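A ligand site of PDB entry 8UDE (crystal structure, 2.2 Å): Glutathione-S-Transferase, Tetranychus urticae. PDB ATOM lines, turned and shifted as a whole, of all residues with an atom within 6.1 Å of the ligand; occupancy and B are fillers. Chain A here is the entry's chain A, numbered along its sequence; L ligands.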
ATOM      1  N   TYR A   7     -19.104   4.442  -8.249  1.00  0.00           N
ATOM      2  CA  TYR A   7     -20.264   3.683  -8.696  1.00  0.00           C
ATOM      3  C   TYR A   7     -19.809   2.505  -9.552  1.00  0.00           C
ATOM      4  O   TYR A   7     -18.640   2.425  -9.905  1.00  0.00           O
ATOM      5  CB  TYR A   7     -21.217   4.554  -9.505  1.00  0.00           C
ATOM      6  CG  TYR A   7     -22.617   3.970  -9.673  1.00  0.00           C
ATOM      7  CD1 TYR A   7     -23.345   3.533  -8.574  1.00  0.00           C
ATOM      8  CD2 TYR A   7     -23.197   3.845 -10.932  1.00  0.00           C
ATOM      9  CE1 TYR A   7     -24.615   2.990  -8.730  1.00  0.00           C
ATOM     10  CE2 TYR A   7     -24.461   3.287 -11.091  1.00  0.00           C
ATOM     11  CZ  TYR A   7     -25.177   2.859  -9.985  1.00  0.00           C
ATOM     12  OH  TYR A   7     -26.444   2.337 -10.171  1.00  0.00           O
ATOM     13  N   TRP A   8     -20.777   1.629  -9.877  1.00  0.00           N
ATOM     14  CA  TRP A   8     -20.629   0.602 -10.867  1.00  0.00           C
ATOM     15  C   TRP A   8     -20.461   1.248 -12.231  1.00  0.00           C
ATOM     16  O   TRP A   8     -20.694   2.443 -12.420  1.00  0.00           O
ATOM     17  CB  TRP A   8     -21.856  -0.342 -10.873  1.00  0.00           C
ATOM     18  CG  TRP A   8     -22.269  -0.819  -9.504  1.00  0.00           C
ATOM     19  CD1 TRP A   8     -23.400  -0.480  -8.825  1.00  0.00           C
ATOM     20  CD2 TRP A   8     -21.569  -1.750  -8.631  1.00  0.00           C
ATOM     21  NE1 TRP A   8     -23.462  -1.104  -7.606  1.00  0.00           N
ATOM     22  CE2 TRP A   8     -22.362  -1.902  -7.478  1.00  0.00           C
ATOM     23  CE3 TRP A   8     -20.375  -2.466  -8.741  1.00  0.00           C
ATOM     24  CZ2 TRP A   8     -21.998  -2.749  -6.425  1.00  0.00           C
ATOM     25  CZ3 TRP A   8     -20.028  -3.319  -7.720  1.00  0.00           C
ATOM     26  CH2 TRP A   8     -20.838  -3.473  -6.589  1.00  0.00           C
ATOM     27  N   ILE A  10     -22.273   1.239 -14.750  1.00  0.00           N
ATOM     28  CA  ILE A  10     -23.597   1.227 -15.378  1.00  0.00           C
ATOM     29  C   ILE A  10     -24.148   2.636 -15.224  1.00  0.00           C
ATOM     30  O   ILE A  10     -23.571   3.423 -14.459  1.00  0.00           O
ATOM     31  CB  ILE A  10     -24.542   0.177 -14.745  1.00  0.00           C
ATOM     32  CG1 ILE A  10     -24.860   0.579 -13.301  1.00  0.00           C
ATOM     33  CG2 ILE A  10     -23.958  -1.220 -14.836  1.00  0.00           C
ATOM     34  CD1 ILE A  10     -25.779  -0.390 -12.560  1.00  0.00           C
ATOM     35  N   ARG A  11     -25.241   2.957 -15.928  1.00  0.00           N
ATOM     36  CA  ARG A  11     -25.902   4.236 -15.725  1.00  0.00           C
ATOM     37  C   ARG A  11     -26.605   4.220 -14.374  1.00  0.00           C
ATOM     38  O   ARG A  11     -26.268   4.977 -13.459  1.00  0.00           O
ATOM     39  CB  ARG A  11     -26.841   4.545 -16.885  1.00  0.00           C
ATOM     40  CG  ARG A  11     -26.106   4.834 -18.192  1.00  0.00           C
ATOM     41  CD  ARG A  11     -27.092   5.102 -19.304  1.00  0.00           C
ATOM     42  NE  ARG A  11     -27.893   6.270 -19.039  1.00  0.00           N
ATOM     43  CZ  ARG A  11     -28.910   6.660 -19.780  1.00  0.00           C
ATOM     44  NH1 ARG A  11     -29.258   5.962 -20.843  1.00  0.00           N
ATOM     45  NH2 ARG A  11     -29.598   7.752 -19.462  1.00  0.00           N
ATOM     46  N   GLY A  12     -27.565   3.298 -14.238  1.00  0.00           N
ATOM     47  CA  GLY A  12     -28.121   2.886 -12.952  1.00  0.00           C
ATOM     48  C   GLY A  12     -28.753   4.055 -12.192  1.00  0.00           C
ATOM     49  O   GLY A  12     -29.343   4.936 -12.815  1.00  0.00           O
ATOM     50  N   LEU A  13     -28.552   4.038 -10.864  1.00  0.00           N
ATOM     51  CA  LEU A  13     -28.996   5.078  -9.934  1.00  0.00           C
ATOM     52  C   LEU A  13     -28.211   6.370 -10.071  1.00  0.00           C
ATOM     53  O   LEU A  13     -28.717   7.435  -9.738  1.00  0.00           O
ATOM     54  CB  LEU A  13     -28.804   4.590  -8.483  1.00  0.00           C
ATOM     55  CG  LEU A  13     -29.726   3.463  -8.067  1.00  0.00           C
ATOM     56  CD1 LEU A  13     -29.389   2.942  -6.679  1.00  0.00           C
ATOM     57  CD2 LEU A  13     -31.160   3.955  -8.104  1.00  0.00           C
ATOM     58  N   ILE A  35     -18.111  -5.284 -12.204  1.00  0.00           N
ATOM     59  CA  ILE A  35     -18.844  -6.480 -11.864  1.00  0.00           C
ATOM     60  C   ILE A  35     -18.360  -7.623 -12.745  1.00  0.00           C
ATOM     61  O   ILE A  35     -18.479  -7.553 -13.971  1.00  0.00           O
ATOM     62  CB  ILE A  35     -20.355  -6.282 -12.017  1.00  0.00           C
ATOM     63  CG1 ILE A  35     -20.844  -5.132 -11.150  1.00  0.00           C
ATOM     64  CG2 ILE A  35     -21.089  -7.597 -11.712  1.00  0.00           C
ATOM     65  CD1 ILE A  35     -22.222  -4.652 -11.496  1.00  0.00           C
ATOM     66  N   TYR A  41     -20.592 -12.979 -10.586  1.00  0.00           N
ATOM     67  CA  TYR A  41     -20.797 -11.538 -10.521  1.00  0.00           C
ATOM     68  C   TYR A  41     -19.867 -10.905  -9.497  1.00  0.00           C
ATOM     69  O   TYR A  41     -20.322 -10.158  -8.634  1.00  0.00           O
ATOM     70  CB  TYR A  41     -22.252 -11.178 -10.193  1.00  0.00           C
ATOM     71  CG  TYR A  41     -23.232 -11.594 -11.285  1.00  0.00           C
ATOM     72  CD1 TYR A  41     -23.079 -11.142 -12.596  1.00  0.00           C
ATOM     73  CD2 TYR A  41     -24.291 -12.460 -11.006  1.00  0.00           C
ATOM     74  CE1 TYR A  41     -23.972 -11.517 -13.579  1.00  0.00           C
ATOM     75  CE2 TYR A  41     -25.209 -12.812 -11.990  1.00  0.00           C
ATOM     76  CZ  TYR A  41     -25.034 -12.354 -13.291  1.00  0.00           C
ATOM     77  OH  TYR A  41     -25.881 -12.680 -14.304  1.00  0.00           O
ATOM     78  N   ILE A  43     -17.644  -8.801  -7.183  1.00  0.00           N
ATOM     79  CA  ILE A  43     -17.613  -7.378  -6.851  1.00  0.00           C
ATOM     80  C   ILE A  43     -16.505  -7.093  -5.856  1.00  0.00           C
ATOM     81  O   ILE A  43     -16.669  -6.244  -4.974  1.00  0.00           O
ATOM     82  CB  ILE A  43     -18.985  -6.914  -6.301  1.00  0.00           C
ATOM     83  CG1 ILE A  43     -19.412  -7.762  -5.107  1.00  0.00           C
ATOM     84  CG2 ILE A  43     -20.021  -6.918  -7.416  1.00  0.00           C
ATOM     85  CD1 ILE A  43     -20.544  -7.148  -4.332  1.00  0.00           C
ATOM     86  N   LEU A  60     -23.110   2.088  -3.070  1.00  0.00           N
ATOM     87  CA  LEU A  60     -22.838   2.863  -4.264  1.00  0.00           C
ATOM     88  C   LEU A  60     -24.134   3.440  -4.824  1.00  0.00           C
ATOM     89  O   LEU A  60     -25.139   2.767  -4.869  1.00  0.00           O
ATOM     90  CB  LEU A  60     -22.100   1.970  -5.261  1.00  0.00           C
ATOM     91  CG  LEU A  60     -20.704   1.533  -4.878  1.00  0.00           C
ATOM     92  CD1 LEU A  60     -20.198   0.481  -5.853  1.00  0.00           C
ATOM     93  CD2 LEU A  60     -19.787   2.718  -4.848  1.00  0.00           C
ATOM     94  N   THR A 110     -38.610   5.605 -10.682  1.00  0.00           N
ATOM     95  CA  THR A 110     -37.279   5.034 -10.693  1.00  0.00           C
ATOM     96  C   THR A 110     -37.246   3.723  -9.896  1.00  0.00           C
ATOM     97  O   THR A 110     -36.706   2.719 -10.385  1.00  0.00           O
ATOM     98  CB  THR A 110     -36.250   6.071 -10.194  1.00  0.00           C
ATOM     99  OG1 THR A 110     -36.344   7.191 -11.064  1.00  0.00           O
ATOM    100  CG2 THR A 110     -34.820   5.591 -10.218  1.00  0.00           C
ATOM    101  N   LEU A 111     -37.898   3.736  -8.730  1.00  0.00           N
ATOM    102  CA  LEU A 111     -37.856   2.588  -7.818  1.00  0.00           C
ATOM    103  C   LEU A 111     -38.729   1.474  -8.359  1.00  0.00           C
ATOM    104  O   LEU A 111     -38.358   0.320  -8.234  1.00  0.00           O
ATOM    105  CB  LEU A 111     -38.275   3.017  -6.415  1.00  0.00           C
ATOM    106  CG  LEU A 111     -37.281   3.921  -5.684  1.00  0.00           C
ATOM    107  CD1 LEU A 111     -37.816   4.307  -4.313  1.00  0.00           C
ATOM    108  CD2 LEU A 111     -35.896   3.294  -5.545  1.00  0.00           C
ATOM    109  N   CYS A 113     -39.101   0.943 -11.584  1.00  0.00           N
ATOM    110  CA  CYS A 113     -38.315   0.393 -12.687  1.00  0.00           C
ATOM    111  C   CYS A 113     -37.177  -0.461 -12.147  1.00  0.00           C
ATOM    112  O   CYS A 113     -36.929  -1.547 -12.664  1.00  0.00           O
ATOM    113  CB  CYS A 113     -37.788   1.480 -13.619  1.00  0.00           C
ATOM    114  SG  CYS A 113     -39.113   2.168 -14.647  1.00  0.00           S
ATOM    115  N   LYS A 114     -36.498   0.021 -11.106  1.00  0.00           N
ATOM    116  CA  LYS A 114     -35.434  -0.734 -10.462  1.00  0.00           C
ATOM    117  C   LYS A 114     -35.928  -2.136 -10.112  1.00  0.00           C
ATOM    118  O   LYS A 114     -35.255  -3.119 -10.436  1.00  0.00           O
ATOM    119  CB  LYS A 114     -34.912  -0.036  -9.211  1.00  0.00           C
ATOM    120  CG  LYS A 114     -33.772  -0.770  -8.493  1.00  0.00           C
ATOM    121  CD  LYS A 114     -33.265  -0.057  -7.250  1.00  0.00           C
ATOM    122  CE  LYS A 114     -31.965  -0.614  -6.722  1.00  0.00           C
ATOM    123  NZ  LYS A 114     -32.190  -1.945  -6.109  1.00  0.00           N
ATOM    124  N   PHE A 117     -36.649  -4.165 -13.482  1.00  0.00           N
ATOM    125  CA  PHE A 117     -35.451  -4.469 -14.260  1.00  0.00           C
ATOM    126  C   PHE A 117     -34.625  -5.578 -13.595  1.00  0.00           C
ATOM    127  O   PHE A 117     -34.011  -6.388 -14.297  1.00  0.00           O
ATOM    128  CB  PHE A 117     -34.604  -3.205 -14.424  1.00  0.00           C
ATOM    129  CG  PHE A 117     -35.207  -2.084 -15.243  1.00  0.00           C
ATOM    130  CD1 PHE A 117     -36.418  -2.233 -15.911  1.00  0.00           C
ATOM    131  CD2 PHE A 117     -34.520  -0.892 -15.387  1.00  0.00           C
ATOM    132  CE1 PHE A 117     -36.960  -1.205 -16.662  1.00  0.00           C
ATOM    133  CE2 PHE A 117     -35.061   0.132 -16.147  1.00  0.00           C
ATOM    134  CZ  PHE A 117     -36.276  -0.038 -16.784  1.00  0.00           C
ATOM    135  N   TYR A 118     -34.643  -5.656 -12.254  1.00  0.00           N
ATOM    136  CA  TYR A 118     -33.864  -6.659 -11.553  1.00  0.00           C
ATOM    137  C   TYR A 118     -34.746  -7.802 -11.050  1.00  0.00           C
ATOM    138  O   TYR A 118     -34.316  -8.570 -10.214  1.00  0.00           O
ATOM    139  CB  TYR A 118     -33.072  -6.030 -10.405  1.00  0.00           C
ATOM    140  CG  TYR A 118     -31.916  -5.144 -10.839  1.00  0.00           C
ATOM    141  CD1 TYR A 118     -30.710  -5.692 -11.265  1.00  0.00           C
ATOM    142  CD2 TYR A 118     -32.037  -3.761 -10.852  1.00  0.00           C
ATOM    143  CE1 TYR A 118     -29.650  -4.897 -11.655  1.00  0.00           C
ATOM    144  CE2 TYR A 118     -30.970  -2.945 -11.240  1.00  0.00           C
ATOM    145  CZ  TYR A 118     -29.772  -3.510 -11.658  1.00  0.00           C
ATOM    146  OH  TYR A 118     -28.739  -2.705 -12.054  1.00  0.00           O
ATOM    147  N   TYR A 171     -34.760   6.048 -19.530  1.00  0.00           N
ATOM    148  CA  TYR A 171     -34.819   4.600 -19.303  1.00  0.00           C
ATOM    149  C   TYR A 171     -36.143   4.035 -19.826  1.00  0.00           C
ATOM    150  O   TYR A 171     -36.174   2.967 -20.426  1.00  0.00           O
ATOM    151  CB  TYR A 171     -34.654   4.199 -17.839  1.00  0.00           C
ATOM    152  CG  TYR A 171     -33.311   4.476 -17.175  1.00  0.00           C
ATOM    153  CD1 TYR A 171     -32.194   4.914 -17.884  1.00  0.00           C
ATOM    154  CD2 TYR A 171     -33.168   4.298 -15.789  1.00  0.00           C
ATOM    155  CE1 TYR A 171     -30.983   5.166 -17.251  1.00  0.00           C
ATOM    156  CE2 TYR A 171     -31.967   4.557 -15.150  1.00  0.00           C
ATOM    157  CZ  TYR A 171     -30.870   5.018 -15.881  1.00  0.00           C
ATOM    158  OH  TYR A 171     -29.678   5.293 -15.271  1.00  0.00           O
ATOM    159  N   ILE A 213     -27.516   0.336 -18.948  1.00  0.00           N
ATOM    160  CA  ILE A 213     -28.422   0.910 -17.942  1.00  0.00           C
ATOM    161  C   ILE A 213     -28.274   0.159 -16.607  1.00  0.00           C
ATOM    162  O   ILE A 213     -28.223   0.774 -15.550  1.00  0.00           O
ATOM    163  CB  ILE A 213     -29.874   0.882 -18.461  1.00  0.00           C
ATOM    164  CG1 ILE A 213     -30.037   1.682 -19.753  1.00  0.00           C
ATOM    165  CG2 ILE A 213     -30.835   1.362 -17.405  1.00  0.00           C
ATOM    166  CD1 ILE A 213     -31.401   1.522 -20.383  1.00  0.00           C
ATOM    167  N   THR A 214     -28.244  -1.184 -16.652  1.00  0.00           N
ATOM    168  CA  THR A 214     -28.310  -1.968 -15.427  1.00  0.00           C
ATOM    169  C   THR A 214     -27.066  -2.855 -15.304  1.00  0.00           C
ATOM    170  O   THR A 214     -26.311  -2.989 -16.255  1.00  0.00           O
ATOM    171  CB  THR A 214     -29.576  -2.813 -15.348  1.00  0.00           C
ATOM    172  OG1 THR A 214     -29.718  -3.500 -16.588  1.00  0.00           O
ATOM    173  CG2 THR A 214     -30.821  -1.986 -15.083  1.00  0.00           C
ATOM    174  N   ALA A 215     -26.909  -3.463 -14.120  1.00  0.00           N
ATOM    175  CA  ALA A 215     -25.905  -4.496 -13.927  1.00  0.00           C
ATOM    176  C   ALA A 215     -26.289  -5.745 -14.724  1.00  0.00           C
ATOM    177  O   ALA A 215     -27.458  -5.901 -15.111  1.00  0.00           O
ATOM    178  CB  ALA A 215     -25.760  -4.784 -12.437  1.00  0.00           C
ATOM    179  N   PRO A 216     -25.336  -6.657 -15.027  1.00  0.00           N
ATOM    180  CA  PRO A 216     -25.582  -7.746 -15.996  1.00  0.00           C
ATOM    181  C   PRO A 216     -26.656  -8.776 -15.623  1.00  0.00           C
ATOM    182  O   PRO A 216     -27.141  -9.449 -16.520  1.00  0.00           O
ATOM    183  CB  PRO A 216     -24.258  -8.503 -16.122  1.00  0.00           C
ATOM    184  CG  PRO A 216     -23.224  -7.628 -15.419  1.00  0.00           C
ATOM    185  CD  PRO A 216     -23.972  -6.711 -14.488  1.00  0.00           C
ATOM    186  N   MET A 217     -27.014  -8.862 -14.325  1.00  0.00           N
ATOM    187  CA  MET A 217     -27.959  -9.884 -13.881  1.00  0.00           C
ATOM    188  C   MET A 217     -29.384  -9.421 -14.146  1.00  0.00           C
ATOM    189  O   MET A 217     -30.300 -10.228 -14.026  1.00  0.00           O
ATOM    190  CB  MET A 217     -27.821 -10.288 -12.395  1.00  0.00           C
ATOM    191  CG  MET A 217     -28.077  -9.176 -11.374  1.00  0.00           C
ATOM    192  SD  MET A 217     -26.852  -7.818 -11.388  1.00  0.00           S
ATOM    193  CE  MET A 217     -25.363  -8.669 -10.858  1.00  0.00           C
HETATM  194  N1  LIG L   1     -30.412   0.244 -12.604  1.00  0.00           N
HETATM  195  C1  LIG L   1     -31.309   0.479 -11.445  1.00  0.00           C
HETATM  196  C2  LIG L   1     -31.932   1.876 -11.566  1.00  0.00           C
HETATM  197  O1  LIG L   1     -31.628   2.549 -12.580  1.00  0.00           O
HETATM  198  O2  LIG L   1     -32.703   2.246 -10.655  1.00  0.00           O
HETATM  199  C3  LIG L   1     -30.537   0.319 -10.133  1.00  0.00           C
HETATM  200  C4  LIG L   1     -29.029   0.301 -10.313  1.00  0.00           C
HETATM  201  C5  LIG L   1     -28.340  -0.487  -9.219  1.00  0.00           C
HETATM  202  O3  LIG L   1     -27.503   0.033  -8.481  1.00  0.00           O
HETATM  203  N2  LIG L   1     -28.704  -1.763  -9.103  1.00  0.00           N
HETATM  204  C6  LIG L   1     -27.939  -2.759  -8.372  1.00  0.00           C
HETATM  205  C7  LIG L   1     -26.553  -3.036  -8.939  1.00  0.00           C
HETATM  206  O4  LIG L   1     -26.140  -2.394  -9.910  1.00  0.00           O
HETATM  207  C8  LIG L   1     -28.696  -4.068  -8.247  1.00  0.00           C
HETATM  208  S1  LIG L   1     -30.300  -3.941  -7.430  1.00  0.00           S
HETATM  209  N3  LIG L   1     -25.845  -4.009  -8.355  1.00  0.00           N
HETATM  210  C9  LIG L   1     -24.518  -4.353  -8.808  1.00  0.00           C
HETATM  211  C10 LIG L   1     -23.934  -5.538  -8.050  1.00  0.00           C
HETATM  212  O5  LIG L   1     -23.600  -6.538  -8.720  1.00  0.00           O
HETATM  213  O6  LIG L   1     -23.833  -5.429  -6.807  1.00  0.00           O
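The side-chain hydroxyl (OH) of Tyr 7 is in hydrogen-bond range of an oxygen (O3) of the ligand, 3.0 Å away. OH of Tyr 118 is in hydrogen-bond range of N2 of the ligand (3.1 Å). The side-chain amino group of Lys 114 lies close to a sulfur (S1) of the ligand.
The backbone carbonyl oxygen (O) of Gly 12 sits at hydrogen-bond distance from the side-chain hydroxyl (OH) of Tyr 171 (2.5 Å). The backbone NH of Gly 12 lies within hydrogen-bond range of the backbone carbonyl oxygen of Ile 213 (2.9 Å). OH of Tyr 118 is in hydrogen-bond range of N of Ala 215, 2.9 Å away. The side-chain hydroxyl of Tyr 7 sits at hydrogen-bond distance from the backbone NH of Leu 13, at 2.8 Å.
An oxygen (O1) of the ligand lies close to the backbone carbonyl oxygen of Gly 12 (3.3 Å). Merely in contact with the ligand: Trp 8 (3.3 Å), Ile 10 (3.3 Å), Leu 13 (3.4 Å), Ile 35 (3.5 Å), Ile 43 (3.8 Å), Thr 110 (3.98 Å), Tyr 171 (3.3 Å), Ile 213 (3.7 Å), Thr 214 (3.4 Å), Ala 215 (3.5 Å) and Met 217 (3.5 Å). Of the 22 residues printed, 15 come within 4 Å of the ligand. The nearest printed residue that does not touch the ligand is Tyr 41 (4.9 Å).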
